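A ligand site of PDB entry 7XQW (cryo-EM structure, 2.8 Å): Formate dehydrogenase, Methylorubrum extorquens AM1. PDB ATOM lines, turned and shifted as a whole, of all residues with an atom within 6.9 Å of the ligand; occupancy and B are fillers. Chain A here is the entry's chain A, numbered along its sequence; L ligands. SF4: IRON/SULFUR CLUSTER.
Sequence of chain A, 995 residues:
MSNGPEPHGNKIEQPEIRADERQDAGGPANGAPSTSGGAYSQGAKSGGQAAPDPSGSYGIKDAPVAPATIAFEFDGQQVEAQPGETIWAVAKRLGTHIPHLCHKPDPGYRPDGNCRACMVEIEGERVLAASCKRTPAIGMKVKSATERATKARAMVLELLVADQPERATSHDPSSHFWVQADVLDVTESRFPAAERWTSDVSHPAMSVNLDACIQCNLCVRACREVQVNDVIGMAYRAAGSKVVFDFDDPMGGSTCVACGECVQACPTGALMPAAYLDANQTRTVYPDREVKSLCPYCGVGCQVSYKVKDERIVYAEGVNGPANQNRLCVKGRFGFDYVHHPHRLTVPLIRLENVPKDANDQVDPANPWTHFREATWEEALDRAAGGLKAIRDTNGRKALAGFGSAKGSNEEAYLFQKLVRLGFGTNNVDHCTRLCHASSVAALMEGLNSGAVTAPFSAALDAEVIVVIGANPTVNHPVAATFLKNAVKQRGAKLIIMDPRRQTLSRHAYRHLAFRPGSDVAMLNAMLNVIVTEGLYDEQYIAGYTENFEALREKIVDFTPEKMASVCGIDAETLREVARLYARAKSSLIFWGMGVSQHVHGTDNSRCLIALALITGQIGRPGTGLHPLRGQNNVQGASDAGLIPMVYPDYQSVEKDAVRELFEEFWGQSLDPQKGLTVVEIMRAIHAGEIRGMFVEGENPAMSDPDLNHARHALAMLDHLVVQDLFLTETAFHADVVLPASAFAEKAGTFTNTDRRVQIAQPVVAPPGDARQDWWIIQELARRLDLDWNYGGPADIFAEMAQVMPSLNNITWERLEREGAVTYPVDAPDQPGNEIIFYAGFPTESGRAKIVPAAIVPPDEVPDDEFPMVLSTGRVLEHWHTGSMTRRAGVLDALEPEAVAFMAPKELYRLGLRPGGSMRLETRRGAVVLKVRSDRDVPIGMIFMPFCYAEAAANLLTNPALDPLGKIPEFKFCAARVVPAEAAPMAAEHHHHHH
N of Cys 216 lies close to S3 of the ligand (3.4 Å).
An iron atom (FE1) of the ligand is bound by the side-chain sulfur (SG) of Cys 216 (2.3 Å).
N of Cys 219 lies close to S2 of the ligand.
SG of Cys 219 binds FE4 of the ligand, at 2.3 Å.
The side-chain sulfur (SG) of Cys 213 is bound to an iron atom (FE2) of the ligand.
FE3 of the ligand is bound by SG of Cys 266, at 2.3 Å.
A sulfur (S4) of the ligand sits close to the backbone NH (N) of Ile 214.
N of Asn 217 sits close to S3 of the ligand (3.3 Å).
S4 of the ligand lies close to OG1 of Thr 268, at 3.5 Å.
The backbone NH (N) of Gln 215 sits close to a sulfur (S3) of the ligand.
The side-chain sulfur of Cys 213 lies close to the backbone NH of Gln 215.
The side-chain sulfur (SG) of Cys 266 lies close to the backbone carbonyl oxygen (O) of Thr 268, 3.3 Å away.
The side-chain sulfur (SG) of Cys 266 sits close to the backbone NH (N) of Leu 271, at 3.5 Å.
OG1 of Thr 268 lies within hydrogen-bond range of N of Ala 270, at 3.1 Å.
The backbone carbonyl oxygen (O) of Ala 212 sits at hydrogen-bond distance from the side-chain hydroxyl (OG1) of Thr 268, 3.5 Å away.
N of Asn 209 lies within hydrogen-bond range of O of Ala 270, 2.8 Å away.
Residues that only touch the ligand: Leu 218, Val 243, Ala 265, Pro 267, Ala 270 and Leu 271.
Hydrophobic or aromatic side chains that line the ligand: Ile 214, Leu 218, Val 243, Pro 267, Ala 270 and Leu 271.
14 residues have an atom within 4 Å of the ligand: Cys 213, Ile 214, Gln 215, Cys 216, Asn 217, Leu 218, Cys 219, Val 243, Ala 265, Cys 266, Pro 267, Thr 268, Ala 270 and Leu 271.
The nearest printed residue that does not touch the ligand is Leu 210 (4.3 Å).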
ATOM      1  N   LEU A 101      23.765 -11.937 -10.185  1.00  0.00           N
ATOM      2  CA  LEU A 101      22.479 -11.689  -9.553  1.00  0.00           C
ATOM      3  C   LEU A 101      22.069 -10.234  -9.665  1.00  0.00           C
ATOM      4  O   LEU A 101      20.955  -9.946 -10.135  1.00  0.00           O
ATOM      5  CB  LEU A 101      22.533 -12.105  -8.071  1.00  0.00           C
ATOM      6  CG  LEU A 101      22.723 -13.597  -7.816  1.00  0.00           C
ATOM      7  CD1 LEU A 101      22.995 -13.852  -6.346  1.00  0.00           C
ATOM      8  CD2 LEU A 101      21.523 -14.394  -8.281  1.00  0.00           C
ATOM      9  N   CYS A 102      22.934  -9.309  -9.262  1.00  0.00           N
ATOM     10  CA  CYS A 102      22.627  -7.894  -9.433  1.00  0.00           C
ATOM     11  C   CYS A 102      22.768  -7.469 -10.881  1.00  0.00           C
ATOM     12  O   CYS A 102      22.055  -6.555 -11.330  1.00  0.00           O
ATOM     13  CB  CYS A 102      23.537  -7.043  -8.532  1.00  0.00           C
ATOM     14  SG  CYS A 102      25.315  -7.201  -8.829  1.00  0.00           S
ATOM     15  N   VAL A 208       4.601  -8.516  -3.854  1.00  0.00           N
ATOM     16  CA  VAL A 208       5.988  -8.396  -3.399  1.00  0.00           C
ATOM     17  C   VAL A 208       6.123  -9.165  -2.090  1.00  0.00           C
ATOM     18  O   VAL A 208       5.367  -8.919  -1.138  1.00  0.00           O
ATOM     19  CB  VAL A 208       6.423  -6.929  -3.229  1.00  0.00           C
ATOM     20  CG1 VAL A 208       5.534  -6.208  -2.244  1.00  0.00           C
ATOM     21  CG2 VAL A 208       7.871  -6.863  -2.780  1.00  0.00           C
ATOM     22  N   ASN A 209       7.075 -10.089  -2.057  1.00  0.00           N
ATOM     23  CA  ASN A 209       7.388 -10.891  -0.866  1.00  0.00           C
ATOM     24  C   ASN A 209       8.880 -10.699  -0.608  1.00  0.00           C
ATOM     25  O   ASN A 209       9.704 -11.464  -1.100  1.00  0.00           O
ATOM     26  CB  ASN A 209       7.032 -12.359  -1.071  1.00  0.00           C
ATOM     27  CG  ASN A 209       5.587 -12.551  -1.472  1.00  0.00           C
ATOM     28  OD1 ASN A 209       4.675 -12.035  -0.833  1.00  0.00           O
ATOM     29  ND2 ASN A 209       5.367 -13.316  -2.539  1.00  0.00           N
ATOM     30  N   LEU A 210       9.215  -9.672   0.174  1.00  0.00           N
ATOM     31  CA  LEU A 210      10.612  -9.308   0.362  1.00  0.00           C
ATOM     32  C   LEU A 210      11.386 -10.346   1.152  1.00  0.00           C
ATOM     33  O   LEU A 210      12.617 -10.270   1.200  1.00  0.00           O
ATOM     34  CB  LEU A 210      10.701  -7.955   1.073  1.00  0.00           C
ATOM     35  CG  LEU A 210      10.160  -6.754   0.300  1.00  0.00           C
ATOM     36  CD1 LEU A 210      10.400  -5.473   1.072  1.00  0.00           C
ATOM     37  CD2 LEU A 210      10.788  -6.673  -1.089  1.00  0.00           C
ATOM     38  N   ALA A 212      12.137 -13.091   0.234  1.00  0.00           N
ATOM     39  CA  ALA A 212      13.049 -13.653  -0.756  1.00  0.00           C
ATOM     40  C   ALA A 212      14.039 -12.624  -1.307  1.00  0.00           C
ATOM     41  O   ALA A 212      14.899 -12.981  -2.113  1.00  0.00           O
ATOM     42  CB  ALA A 212      12.269 -14.270  -1.915  1.00  0.00           C
ATOM     43  N   CYS A 213      13.931 -11.360  -0.882  1.00  0.00           N
ATOM     44  CA  CYS A 213      14.705 -10.300  -1.502  1.00  0.00           C
ATOM     45  C   CYS A 213      16.201 -10.508  -1.289  1.00  0.00           C
ATOM     46  O   CYS A 213      16.641 -10.963  -0.225  1.00  0.00           O
ATOM     47  CB  CYS A 213      14.286  -8.952  -0.925  1.00  0.00           C
ATOM     48  SG  CYS A 213      15.111  -7.529  -1.666  1.00  0.00           S
ATOM     49  N   ILE A 214      16.987 -10.152  -2.307  1.00  0.00           N
ATOM     50  CA  ILE A 214      18.439 -10.279  -2.286  1.00  0.00           C
ATOM     51  C   ILE A 214      19.132  -8.934  -2.120  1.00  0.00           C
ATOM     52  O   ILE A 214      20.360  -8.892  -1.960  1.00  0.00           O
ATOM     53  CB  ILE A 214      18.929 -10.978  -3.567  1.00  0.00           C
ATOM     54  CG1 ILE A 214      18.307 -12.363  -3.705  1.00  0.00           C
ATOM     55  CG2 ILE A 214      20.442 -11.093  -3.591  1.00  0.00           C
ATOM     56  CD1 ILE A 214      18.631 -13.304  -2.600  1.00  0.00           C
ATOM     57  N   GLN A 215      18.377  -7.839  -2.131  1.00  0.00           N
ATOM     58  CA  GLN A 215      18.946  -6.490  -2.152  1.00  0.00           C
ATOM     59  C   GLN A 215      19.893  -6.294  -3.331  1.00  0.00           C
ATOM     60  O   GLN A 215      20.873  -5.565  -3.242  1.00  0.00           O
ATOM     61  CB  GLN A 215      19.662  -6.145  -0.842  1.00  0.00           C
ATOM     62  CG  GLN A 215      18.773  -5.996   0.377  1.00  0.00           C
ATOM     63  CD  GLN A 215      18.593  -7.282   1.152  1.00  0.00           C
ATOM     64  OE1 GLN A 215      19.365  -8.231   0.997  1.00  0.00           O
ATOM     65  NE2 GLN A 215      17.576  -7.321   1.999  1.00  0.00           N
ATOM     66  N   CYS A 216      19.595  -6.950  -4.459  1.00  0.00           N
ATOM     67  CA  CYS A 216      20.422  -6.783  -5.647  1.00  0.00           C
ATOM     68  C   CYS A 216      20.201  -5.434  -6.323  1.00  0.00           C
ATOM     69  O   CYS A 216      20.968  -5.087  -7.225  1.00  0.00           O
ATOM     70  CB  CYS A 216      20.144  -7.917  -6.642  1.00  0.00           C
ATOM     71  SG  CYS A 216      18.489  -7.926  -7.322  1.00  0.00           S
ATOM     72  N   ASN A 217      19.175  -4.686  -5.928  1.00  0.00           N
ATOM     73  CA  ASN A 217      18.947  -3.296  -6.289  1.00  0.00           C
ATOM     74  C   ASN A 217      18.344  -3.172  -7.694  1.00  0.00           C
ATOM     75  O   ASN A 217      18.058  -2.061  -8.132  1.00  0.00           O
ATOM     76  CB  ASN A 217      20.245  -2.484  -6.199  1.00  0.00           C
ATOM     77  CG  ASN A 217      20.031  -0.991  -6.346  1.00  0.00           C
ATOM     78  OD1 ASN A 217      18.929  -0.528  -6.543  1.00  0.00           O
ATOM     79  ND2 ASN A 217      21.123  -0.242  -6.253  1.00  0.00           N
ATOM     80  N   LEU A 218      18.135  -4.285  -8.406  1.00  0.00           N
ATOM     81  CA  LEU A 218      17.663  -4.193  -9.786  1.00  0.00           C
ATOM     82  C   LEU A 218      16.325  -3.483  -9.885  1.00  0.00           C
ATOM     83  O   LEU A 218      16.052  -2.792 -10.880  1.00  0.00           O
ATOM     84  CB  LEU A 218      17.563  -5.591 -10.404  1.00  0.00           C
ATOM     85  CG  LEU A 218      18.817  -6.129 -11.083  1.00  0.00           C
ATOM     86  CD1 LEU A 218      18.644  -7.600 -11.410  1.00  0.00           C
ATOM     87  CD2 LEU A 218      19.136  -5.349 -12.345  1.00  0.00           C
ATOM     88  N   CYS A 219      15.455  -3.638  -8.877  1.00  0.00           N
ATOM     89  CA  CYS A 219      14.142  -3.021  -8.947  1.00  0.00           C
ATOM     90  C   CYS A 219      14.230  -1.500  -8.871  1.00  0.00           C
ATOM     91  O   CYS A 219      13.432  -0.792  -9.494  1.00  0.00           O
ATOM     92  CB  CYS A 219      13.252  -3.568  -7.834  1.00  0.00           C
ATOM     93  SG  CYS A 219      13.989  -3.557  -6.192  1.00  0.00           S
ATOM     94  N   VAL A 220      15.189  -0.978  -8.097  1.00  0.00           N
ATOM     95  CA  VAL A 220      15.333   0.464  -7.995  1.00  0.00           C
ATOM     96  C   VAL A 220      15.837   1.033  -9.317  1.00  0.00           C
ATOM     97  O   VAL A 220      15.419   2.098  -9.754  1.00  0.00           O
ATOM     98  CB  VAL A 220      16.267   0.836  -6.825  1.00  0.00           C
ATOM     99  CG1 VAL A 220      16.224   2.339  -6.567  1.00  0.00           C
ATOM    100  CG2 VAL A 220      15.932   0.049  -5.563  1.00  0.00           C
ATOM    101  N   ILE A 232      10.568   3.489  -6.038  1.00  0.00           N
ATOM    102  CA  ILE A 232      11.267   2.422  -5.330  1.00  0.00           C
ATOM    103  C   ILE A 232      12.576   2.974  -4.784  1.00  0.00           C
ATOM    104  O   ILE A 232      13.175   3.880  -5.351  1.00  0.00           O
ATOM    105  CB  ILE A 232      11.517   1.196  -6.255  1.00  0.00           C
ATOM    106  CG1 ILE A 232      10.248   0.348  -6.346  1.00  0.00           C
ATOM    107  CG2 ILE A 232      12.683   0.358  -5.742  1.00  0.00           C
ATOM    108  CD1 ILE A 232      10.424  -0.942  -7.118  1.00  0.00           C
ATOM    109  N   MET A 234      16.012   1.671  -1.709  1.00  0.00           N
ATOM    110  CA  MET A 234      16.504   0.903  -0.538  1.00  0.00           C
ATOM    111  C   MET A 234      16.763   1.951   0.542  1.00  0.00           C
ATOM    112  O   MET A 234      17.812   2.602   0.479  1.00  0.00           O
ATOM    113  CB  MET A 234      17.806   0.174  -0.866  1.00  0.00           C
ATOM    114  CG  MET A 234      18.264  -0.788   0.207  1.00  0.00           C
ATOM    115  SD  MET A 234      17.358  -2.361   0.156  1.00  0.00           S
ATOM    116  CE  MET A 234      17.622  -2.837  -1.553  1.00  0.00           C
ATOM    117  N   VAL A 243      13.579  -3.078   0.333  1.00  0.00           N
ATOM    118  CA  VAL A 243      12.981  -2.408  -0.807  1.00  0.00           C
ATOM    119  C   VAL A 243      11.701  -1.733  -0.335  1.00  0.00           C
ATOM    120  O   VAL A 243      10.819  -2.385   0.250  1.00  0.00           O
ATOM    121  CB  VAL A 243      12.700  -3.389  -1.948  1.00  0.00           C
ATOM    122  CG1 VAL A 243      12.009  -2.683  -3.108  1.00  0.00           C
ATOM    123  CG2 VAL A 243      13.991  -4.045  -2.415  1.00  0.00           C
ATOM    124  N   CYS A 262      10.051  -3.595 -12.577  1.00  0.00           N
ATOM    125  CA  CYS A 262      10.736  -4.223 -11.451  1.00  0.00           C
ATOM    126  C   CYS A 262      10.470  -5.721 -11.408  1.00  0.00           C
ATOM    127  O   CYS A 262      11.392  -6.518 -11.201  1.00  0.00           O
ATOM    128  CB  CYS A 262      10.283  -3.558 -10.150  1.00  0.00           C
ATOM    129  SG  CYS A 262       8.511  -3.632  -9.881  1.00  0.00           S
ATOM    130  N   ALA A 265      12.507  -7.398 -13.501  1.00  0.00           N
ATOM    131  CA  ALA A 265      13.930  -7.111 -13.186  1.00  0.00           C
ATOM    132  C   ALA A 265      14.370  -7.877 -11.937  1.00  0.00           C
ATOM    133  O   ALA A 265      15.562  -7.811 -11.601  1.00  0.00           O
ATOM    134  CB  ALA A 265      14.137  -5.633 -13.032  1.00  0.00           C
ATOM    135  N   CYS A 266      13.440  -8.579 -11.265  1.00  0.00           N
ATOM    136  CA  CYS A 266      13.792  -9.280 -10.040  1.00  0.00           C
ATOM    137  C   CYS A 266      14.427 -10.631 -10.367  1.00  0.00           C
ATOM    138  O   CYS A 266      13.842 -11.419 -11.122  1.00  0.00           O
ATOM    139  CB  CYS A 266      12.559  -9.468  -9.168  1.00  0.00           C
ATOM    140  SG  CYS A 266      12.916 -10.005  -7.482  1.00  0.00           S
ATOM    141  N   PRO A 267      15.608 -10.932  -9.824  1.00  0.00           N
ATOM    142  CA  PRO A 267      16.204 -12.248 -10.042  1.00  0.00           C
ATOM    143  C   PRO A 267      15.680 -13.318  -9.107  1.00  0.00           C
ATOM    144  O   PRO A 267      16.034 -14.495  -9.267  1.00  0.00           O
ATOM    145  CB  PRO A 267      17.696 -11.988  -9.810  1.00  0.00           C
ATOM    146  CG  PRO A 267      17.717 -10.879  -8.831  1.00  0.00           C
ATOM    147  CD  PRO A 267      16.502 -10.040  -9.073  1.00  0.00           C
ATOM    148  N   THR A 268      14.860 -12.952  -8.130  1.00  0.00           N
ATOM    149  CA  THR A 268      14.189 -13.887  -7.244  1.00  0.00           C
ATOM    150  C   THR A 268      12.683 -13.774  -7.478  1.00  0.00           C
ATOM    151  O   THR A 268      12.215 -13.069  -8.366  1.00  0.00           O
ATOM    152  CB  THR A 268      14.544 -13.602  -5.779  1.00  0.00           C
ATOM    153  OG1 THR A 268      13.991 -12.338  -5.381  1.00  0.00           O
ATOM    154  CG2 THR A 268      16.035 -13.575  -5.582  1.00  0.00           C
ATOM    155  N   GLY A 269      11.918 -14.495  -6.660  1.00  0.00           N
ATOM    156  CA  GLY A 269      10.484 -14.348  -6.656  1.00  0.00           C
ATOM    157  C   GLY A 269       9.992 -13.261  -5.737  1.00  0.00           C
ATOM    158  O   GLY A 269       8.787 -13.199  -5.469  1.00  0.00           O
ATOM    159  N   ALA A 270      10.884 -12.408  -5.237  1.00  0.00           N
ATOM    160  CA  ALA A 270      10.461 -11.339  -4.343  1.00  0.00           C
ATOM    161  C   ALA A 270       9.451 -10.423  -5.020  1.00  0.00           C
ATOM    162  O   ALA A 270       8.573  -9.879  -4.357  1.00  0.00           O
ATOM    163  CB  ALA A 270      11.669 -10.532  -3.873  1.00  0.00           C
ATOM    164  N   LEU A 271       9.580 -10.231  -6.324  1.00  0.00           N
ATOM    165  CA  LEU A 271       8.620  -9.488  -7.124  1.00  0.00           C
ATOM    166  C   LEU A 271       8.112 -10.408  -8.223  1.00  0.00           C
ATOM    167  O   LEU A 271       8.872 -10.808  -9.101  1.00  0.00           O
ATOM    168  CB  LEU A 271       9.251  -8.232  -7.724  1.00  0.00           C
ATOM    169  CG  LEU A 271       9.567  -7.089  -6.752  1.00  0.00           C
ATOM    170  CD1 LEU A 271      10.203  -5.940  -7.500  1.00  0.00           C
ATOM    171  CD2 LEU A 271       8.320  -6.617  -6.027  1.00  0.00           C
HETATM  172 FE1  SF4 L   1      16.613  -7.449  -6.165  1.00  0.00          FE
HETATM  173 FE2  SF4 L   1      15.044  -7.553  -3.931  1.00  0.00          FE
HETATM  174 FE3  SF4 L   1      14.062  -8.418  -6.325  1.00  0.00          FE
HETATM  175 FE4  SF4 L   1      14.484  -5.744  -5.909  1.00  0.00          FE
HETATM  176  S1  SF4 L   1      12.996  -7.084  -4.813  1.00  0.00           S
HETATM  177  S2  SF4 L   1      15.059  -6.942  -7.763  1.00  0.00           S
HETATM  178  S3  SF4 L   1      16.353  -5.811  -4.603  1.00  0.00           S
HETATM  179  S4  SF4 L   1      15.796  -9.315  -5.154  1.00  0.00           S
